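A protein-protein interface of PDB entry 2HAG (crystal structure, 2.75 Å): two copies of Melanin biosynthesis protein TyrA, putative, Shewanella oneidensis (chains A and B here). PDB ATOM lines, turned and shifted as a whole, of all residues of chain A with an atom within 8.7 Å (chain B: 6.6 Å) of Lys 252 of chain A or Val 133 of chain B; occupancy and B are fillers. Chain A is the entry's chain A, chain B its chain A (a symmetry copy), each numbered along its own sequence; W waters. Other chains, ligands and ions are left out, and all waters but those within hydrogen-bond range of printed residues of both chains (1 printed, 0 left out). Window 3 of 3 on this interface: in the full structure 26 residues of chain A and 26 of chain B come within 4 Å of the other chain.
The side-chain amino group (NZ) of Lys 252 of chain A sits at hydrogen-bond distance from the backbone carbonyl oxygen (O) of Val 133 of chain B. The side-chain hydroxyl (OG) of Ser 250 of chain A sits at hydrogen-bond distance from the side-chain carboxylate (OE1) of Glu 135 of chain B (3.0 Å). OE1 of Glu 135 of chain B lies within hydrogen-bond range of N of Leu 251 of chain A.
The backbone carbonyl oxygen (O) of Met 26 of chain B is in hydrogen-bond range of the backbone NH (N) of Val 133 of chain B, 2.7 Å away. N of Lys 252 of chain A lies close to OG of Ser 250 of chain A, at 3.3 Å.
Among the printed residues, pairs that only touch across the chains: Leu 251 of chain A with Leu 132 of chain B (3.7 Å), Leu 251 of chain A with Leu 25 of chain B (3.7 Å) and Lys 252 of chain A with Glu 135 of chain B (3.9 Å).
Printed residues of chain B within 4 Å of Lys 252 of chain A: Val 133 (3.4 Å) and Glu 135 (3.9 Å). Of the printed residues of chain A, Val 133 of chain B touches Lys 252. Of chain A, only Leu 251 (3.7 Å) comes within 4 Å of Leu 132 of chain B. Printed residues of chain B within 4 Å of Leu 251 of chain A: Leu 25 (3.7 Å), Leu 132 (3.7 Å) and Glu 135 (3.0 Å). Printed residues of chain A within 4 Å of Leu 25 of chain B: Leu 251 (3.7 Å). Of the printed residues of chain A, Glu 135 of chain B touches Ser 250 (3.0 Å), Leu 251 (3.0 Å) and Lys 252 (3.9 Å). Of the printed residues of chain B, Ser 250 of chain A touches Glu 135. Leu 294 of chain A touches none of the printed residues of chain B. Met 26 of chain B touches none of the printed residues of chain A. The nearest residue of chain A that does not touch Val 133 of chain B is Leu 251 of chain A (8.0 Å).
Printed residues of chain A that touch a printed residue of chain B: Ser 250, Leu 251 and Lys 252. Among the printed residues, no Asp or Glu carboxylate lies within 4 Å of a Lys or Arg side-chain nitrogen of the other chain.
No position is printed for both chains. Of the 6 pairs that touch across the chains among the printed residues, none has its exchanged pair printed and touching as well.
Water W1 lies within hydrogen-bond range of the side-chain amino group (NZ) of Lys 252 of chain A, the backbone carbonyl oxygen (O) of Leu 132 of chain B and the backbone carbonyl oxygen (O) of Val 133 of chain B.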
ATOM      1  N   ALA A 187      -4.269  35.226  -1.312  1.00  0.00           N
ATOM      2  CA  ALA A 187      -3.589  34.519  -0.240  1.00  0.00           C
ATOM      3  C   ALA A 187      -4.212  34.914   1.087  1.00  0.00           C
ATOM      4  O   ALA A 187      -4.080  36.060   1.537  1.00  0.00           O
ATOM      5  CB  ALA A 187      -2.118  34.844  -0.246  1.00  0.00           C
ATOM      6  N   HIS A 188      -4.898  33.963   1.711  1.00  0.00           N
ATOM      7  CA  HIS A 188      -5.581  34.232   2.960  1.00  0.00           C
ATOM      8  C   HIS A 188      -4.605  34.278   4.103  1.00  0.00           C
ATOM      9  O   HIS A 188      -3.687  33.469   4.187  1.00  0.00           O
ATOM     10  CB  HIS A 188      -6.604  33.149   3.265  1.00  0.00           C
ATOM     11  CG  HIS A 188      -7.779  33.147   2.344  1.00  0.00           C
ATOM     12  ND1 HIS A 188      -7.681  33.475   1.012  1.00  0.00           N
ATOM     13  CD2 HIS A 188      -9.075  32.821   2.560  1.00  0.00           C
ATOM     14  CE1 HIS A 188      -8.869  33.362   0.450  1.00  0.00           C
ATOM     15  NE2 HIS A 188      -9.731  32.963   1.367  1.00  0.00           N
ATOM     16  N   TYR A 248      -6.935  26.780  -2.880  1.00  0.00           N
ATOM     17  CA  TYR A 248      -5.657  26.298  -3.397  1.00  0.00           C
ATOM     18  C   TYR A 248      -4.583  26.405  -2.338  1.00  0.00           C
ATOM     19  O   TYR A 248      -4.767  27.045  -1.296  1.00  0.00           O
ATOM     20  CB  TYR A 248      -5.194  27.139  -4.581  1.00  0.00           C
ATOM     21  CG  TYR A 248      -4.452  28.387  -4.151  1.00  0.00           C
ATOM     22  CD1 TYR A 248      -5.145  29.519  -3.739  1.00  0.00           C
ATOM     23  CD2 TYR A 248      -3.058  28.433  -4.146  1.00  0.00           C
ATOM     24  CE1 TYR A 248      -4.479  30.656  -3.346  1.00  0.00           C
ATOM     25  CE2 TYR A 248      -2.377  29.575  -3.744  1.00  0.00           C
ATOM     26  CZ  TYR A 248      -3.097  30.681  -3.342  1.00  0.00           C
ATOM     27  OH  TYR A 248      -2.447  31.822  -2.932  1.00  0.00           O
ATOM     28  N   GLY A 249      -3.445  25.788  -2.625  1.00  0.00           N
ATOM     29  CA  GLY A 249      -2.232  26.075  -1.887  1.00  0.00           C
ATOM     30  C   GLY A 249      -1.914  25.092  -0.786  1.00  0.00           C
ATOM     31  O   GLY A 249      -2.504  24.009  -0.701  1.00  0.00           O
ATOM     32  N   SER A 250      -0.961  25.495   0.051  1.00  0.00           N
ATOM     33  CA  SER A 250      -0.420  24.663   1.099  1.00  0.00           C
ATOM     34  C   SER A 250      -0.035  25.586   2.258  1.00  0.00           C
ATOM     35  O   SER A 250      -0.365  26.771   2.240  1.00  0.00           O
ATOM     36  CB  SER A 250       0.807  23.906   0.576  1.00  0.00           C
ATOM     37  OG  SER A 250       2.012  24.632   0.824  1.00  0.00           O
ATOM     38  N   LEU A 251       0.669  25.066   3.255  1.00  0.00           N
ATOM     39  CA  LEU A 251       0.998  25.873   4.415  1.00  0.00           C
ATOM     40  C   LEU A 251       1.762  27.107   4.008  1.00  0.00           C
ATOM     41  O   LEU A 251       1.559  28.162   4.580  1.00  0.00           O
ATOM     42  CB  LEU A 251       1.831  25.088   5.421  1.00  0.00           C
ATOM     43  CG  LEU A 251       1.146  23.948   6.177  1.00  0.00           C
ATOM     44  CD1 LEU A 251       2.196  23.109   6.869  1.00  0.00           C
ATOM     45  CD2 LEU A 251       0.141  24.464   7.192  1.00  0.00           C
ATOM     46  N   LYS A 252       2.636  26.982   3.016  1.00  0.00           N
ATOM     47  CA  LYS A 252       3.516  28.094   2.629  1.00  0.00           C
ATOM     48  C   LYS A 252       2.673  29.274   2.162  1.00  0.00           C
ATOM     49  O   LYS A 252       3.046  30.424   2.323  1.00  0.00           O
ATOM     50  CB  LYS A 252       4.505  27.673   1.524  1.00  0.00           C
ATOM     51  CG  LYS A 252       5.251  26.338   1.789  1.00  0.00           C
ATOM     52  CD  LYS A 252       6.489  26.134   0.886  1.00  0.00           C
ATOM     53  CE  LYS A 252       7.079  24.718   1.042  1.00  0.00           C
ATOM     54  NZ  LYS A 252       8.575  24.671   0.945  1.00  0.00           N
ATOM     55  N   GLU A 253       1.519  28.979   1.590  1.00  0.00           N
ATOM     56  CA  GLU A 253       0.655  30.015   1.061  1.00  0.00           C
ATOM     57  C   GLU A 253      -0.605  29.357   0.533  1.00  0.00           C
ATOM     58  O   GLU A 253      -0.543  28.458  -0.309  1.00  0.00           O
ATOM     59  CB  GLU A 253       1.363  30.771  -0.058  1.00  0.00           C
ATOM     60  CG  GLU A 253       0.457  31.646  -0.888  1.00  0.00           C
ATOM     61  CD  GLU A 253       1.076  31.984  -2.225  1.00  0.00           C
ATOM     62  OE1 GLU A 253       2.212  32.509  -2.255  1.00  0.00           O
ATOM     63  OE2 GLU A 253       0.427  31.706  -3.248  1.00  0.00           O
ATOM     64  N   GLN A 254      -1.744  29.806   1.040  1.00  0.00           N
ATOM     65  CA  GLN A 254      -3.029  29.222   0.673  1.00  0.00           C
ATOM     66  C   GLN A 254      -4.121  30.284   0.600  1.00  0.00           C
ATOM     67  O   GLN A 254      -4.010  31.359   1.200  1.00  0.00           O
ATOM     68  CB  GLN A 254      -3.430  28.158   1.698  1.00  0.00           C
ATOM     69  CG  GLN A 254      -3.621  28.709   3.098  1.00  0.00           C
ATOM     70  CD  GLN A 254      -3.651  27.625   4.141  1.00  0.00           C
ATOM     71  OE1 GLN A 254      -4.565  26.805   4.167  1.00  0.00           O
ATOM     72  NE2 GLN A 254      -2.647  27.610   5.010  1.00  0.00           N
ATOM     73  N   GLY A 255      -5.190  29.965  -0.117  1.00  0.00           N
ATOM     74  CA  GLY A 255      -6.324  30.854  -0.173  1.00  0.00           C
ATOM     75  C   GLY A 255      -7.319  30.448  -1.230  1.00  0.00           C
ATOM     76  O   GLY A 255      -7.699  29.288  -1.319  1.00  0.00           O
ATOM     77  N   LEU A 294      -2.331  38.356  -4.792  1.00  0.00           N
ATOM     78  CA  LEU A 294      -0.932  38.418  -5.204  1.00  0.00           C
ATOM     79  C   LEU A 294      -0.804  38.551  -6.719  1.00  0.00           C
ATOM     80  O   LEU A 294       0.201  39.040  -7.222  1.00  0.00           O
ATOM     81  CB  LEU A 294      -0.171  37.177  -4.727  1.00  0.00           C
ATOM     82  CG  LEU A 294      -0.327  36.799  -3.248  1.00  0.00           C
ATOM     83  CD1 LEU A 294       0.457  35.531  -2.904  1.00  0.00           C
ATOM     84  CD2 LEU A 294       0.105  37.943  -2.360  1.00  0.00           C
ATOM     85  N   LEU B  25       5.385  16.753   5.805  1.00  0.00           N
ATOM     86  CA  LEU B  25       5.885  17.994   6.382  1.00  0.00           C
ATOM     87  C   LEU B  25       7.209  17.800   7.090  1.00  0.00           C
ATOM     88  O   LEU B  25       7.313  16.949   7.975  1.00  0.00           O
ATOM     89  CB  LEU B  25       4.888  18.520   7.403  1.00  0.00           C
ATOM     90  CG  LEU B  25       3.456  18.703   6.928  1.00  0.00           C
ATOM     91  CD1 LEU B  25       2.577  19.116   8.084  1.00  0.00           C
ATOM     92  CD2 LEU B  25       3.403  19.735   5.827  1.00  0.00           C
ATOM     93  N   MET B  26       8.203  18.621   6.728  1.00  0.00           N
ATOM     94  CA  MET B  26       9.520  18.623   7.393  1.00  0.00           C
ATOM     95  C   MET B  26       9.713  19.907   8.141  1.00  0.00           C
ATOM     96  O   MET B  26       9.725  20.981   7.545  1.00  0.00           O
ATOM     97  CB  MET B  26      10.676  18.550   6.405  1.00  0.00           C
ATOM     98  CG  MET B  26      10.386  17.812   5.147  1.00  0.00           C
ATOM     99  SD  MET B  26      10.050  15.953   5.471  1.00  0.00           S
ATOM    100  CE  MET B  26       9.445  15.505   3.574  1.00  0.00           C
ATOM    101  N   PHE B  27       9.895  19.797   9.446  1.00  0.00           N
ATOM    102  CA  PHE B  27      10.172  20.954  10.252  1.00  0.00           C
ATOM    103  C   PHE B  27      11.578  20.847  10.766  1.00  0.00           C
ATOM    104  O   PHE B  27      12.076  19.748  10.973  1.00  0.00           O
ATOM    105  CB  PHE B  27       9.234  21.010  11.445  1.00  0.00           C
ATOM    106  CG  PHE B  27       7.795  21.049  11.078  1.00  0.00           C
ATOM    107  CD1 PHE B  27       7.168  22.249  10.835  1.00  0.00           C
ATOM    108  CD2 PHE B  27       7.064  19.885  10.994  1.00  0.00           C
ATOM    109  CE1 PHE B  27       5.839  22.288  10.505  1.00  0.00           C
ATOM    110  CE2 PHE B  27       5.731  19.918  10.666  1.00  0.00           C
ATOM    111  CZ  PHE B  27       5.117  21.119  10.420  1.00  0.00           C
ATOM    112  N   ASN B  28      12.211  21.995  10.959  1.00  0.00           N
ATOM    113  CA  ASN B  28      13.410  22.076  11.760  1.00  0.00           C
ATOM    114  C   ASN B  28      13.096  22.933  12.955  1.00  0.00           C
ATOM    115  O   ASN B  28      12.321  23.884  12.861  1.00  0.00           O
ATOM    116  CB  ASN B  28      14.575  22.654  10.967  1.00  0.00           C
ATOM    117  CG  ASN B  28      15.192  21.639  10.048  1.00  0.00           C
ATOM    118  OD1 ASN B  28      15.081  20.446  10.283  1.00  0.00           O
ATOM    119  ND2 ASN B  28      15.833  22.099   8.990  1.00  0.00           N
ATOM    120  N   TYR B 101      16.179  16.348   8.567  1.00  0.00           N
ATOM    121  CA  TYR B 101      15.251  17.326   9.101  1.00  0.00           C
ATOM    122  C   TYR B 101      14.945  16.941  10.535  1.00  0.00           C
ATOM    123  O   TYR B 101      14.867  15.752  10.862  1.00  0.00           O
ATOM    124  CB  TYR B 101      13.957  17.354   8.285  1.00  0.00           C
ATOM    125  CG  TYR B 101      14.141  17.644   6.804  1.00  0.00           C
ATOM    126  CD1 TYR B 101      14.415  18.930   6.355  1.00  0.00           C
ATOM    127  CD2 TYR B 101      14.013  16.630   5.853  1.00  0.00           C
ATOM    128  CE1 TYR B 101      14.575  19.198   5.000  1.00  0.00           C
ATOM    129  CE2 TYR B 101      14.170  16.886   4.493  1.00  0.00           C
ATOM    130  CZ  TYR B 101      14.452  18.170   4.071  1.00  0.00           C
ATOM    131  OH  TYR B 101      14.606  18.430   2.724  1.00  0.00           O
ATOM    132  N   GLU B 131      10.121  25.607  12.210  1.00  0.00           N
ATOM    133  CA  GLU B 131       9.964  26.220  10.894  1.00  0.00           C
ATOM    134  C   GLU B 131       9.733  25.120   9.890  1.00  0.00           C
ATOM    135  O   GLU B 131      10.500  24.162   9.830  1.00  0.00           O
ATOM    136  CB  GLU B 131      11.214  26.994  10.469  1.00  0.00           C
ATOM    137  CG  GLU B 131      11.629  28.120  11.408  1.00  0.00           C
ATOM    138  CD  GLU B 131      10.655  29.289  11.404  1.00  0.00           C
ATOM    139  OE1 GLU B 131       9.983  29.500  10.372  1.00  0.00           O
ATOM    140  OE2 GLU B 131      10.564  29.996  12.436  1.00  0.00           O
ATOM    141  N   LEU B 132       8.674  25.257   9.107  1.00  0.00           N
ATOM    142  CA  LEU B 132       8.416  24.344   8.011  1.00  0.00           C
ATOM    143  C   LEU B 132       9.463  24.564   6.944  1.00  0.00           C
ATOM    144  O   LEU B 132       9.600  25.659   6.426  1.00  0.00           O
ATOM    145  CB  LEU B 132       7.036  24.604   7.419  1.00  0.00           C
ATOM    146  CG  LEU B 132       6.659  23.751   6.211  1.00  0.00           C
ATOM    147  CD1 LEU B 132       6.337  22.325   6.654  1.00  0.00           C
ATOM    148  CD2 LEU B 132       5.481  24.367   5.476  1.00  0.00           C
ATOM    149  N   VAL B 133      10.202  23.521   6.611  1.00  0.00           N
ATOM    150  CA  VAL B 133      11.274  23.638   5.634  1.00  0.00           C
ATOM    151  C   VAL B 133      10.779  23.138   4.283  1.00  0.00           C
ATOM    152  O   VAL B 133      10.918  23.818   3.266  1.00  0.00           O
ATOM    153  CB  VAL B 133      12.509  22.818   6.055  1.00  0.00           C
ATOM    154  CG1 VAL B 133      13.690  23.153   5.169  1.00  0.00           C
ATOM    155  CG2 VAL B 133      12.843  23.069   7.508  1.00  0.00           C
ATOM    156  N   GLU B 134      10.206  21.938   4.278  1.00  0.00           N
ATOM    157  CA  GLU B 134       9.679  21.363   3.053  1.00  0.00           C
ATOM    158  C   GLU B 134       8.269  20.836   3.282  1.00  0.00           C
ATOM    159  O   GLU B 134       7.949  20.312   4.349  1.00  0.00           O
ATOM    160  CB  GLU B 134      10.583  20.237   2.528  1.00  0.00           C
ATOM    161  CG  GLU B 134      12.045  20.614   2.347  1.00  0.00           C
ATOM    162  CD  GLU B 134      12.245  21.696   1.311  1.00  0.00           C
ATOM    163  OE1 GLU B 134      11.431  21.781   0.372  1.00  0.00           O
ATOM    164  OE2 GLU B 134      13.222  22.464   1.434  1.00  0.00           O
ATOM    165  N   GLU B 135       7.433  21.019   2.268  1.00  0.00           N
ATOM    166  CA  GLU B 135       6.120  20.419   2.215  1.00  0.00           C
ATOM    167  C   GLU B 135       5.918  19.806   0.849  1.00  0.00           C
ATOM    168  O   GLU B 135       6.227  20.426  -0.167  1.00  0.00           O
ATOM    169  CB  GLU B 135       5.027  21.457   2.439  1.00  0.00           C
ATOM    170  CG  GLU B 135       3.646  20.922   2.053  1.00  0.00           C
ATOM    171  CD  GLU B 135       2.501  21.649   2.728  1.00  0.00           C
ATOM    172  OE1 GLU B 135       2.682  22.841   3.087  1.00  0.00           O
ATOM    173  OE2 GLU B 135       1.425  21.024   2.884  1.00  0.00           O
ATOM    174  N   GLU B 136       5.389  18.591   0.831  1.00  0.00           N
ATOM    175  CA  GLU B 136       5.017  17.921  -0.404  1.00  0.00           C
ATOM    176  C   GLU B 136       3.718  17.177  -0.168  1.00  0.00           C
ATOM    177  O   GLU B 136       3.433  16.723   0.943  1.00  0.00           O
ATOM    178  CB  GLU B 136       6.109  16.944  -0.849  1.00  0.00           C
ATOM    179  CG  GLU B 136       7.473  17.588  -1.084  1.00  0.00           C
ATOM    180  CD  GLU B 136       7.548  18.444  -2.344  1.00  0.00           C
ATOM    181  OE1 GLU B 136       6.555  18.484  -3.111  1.00  0.00           O
ATOM    182  OE2 GLU B 136       8.610  19.069  -2.578  1.00  0.00           O
HETATM  183  O   HOH W   1       8.451  26.264   3.225  1.00  0.00           O
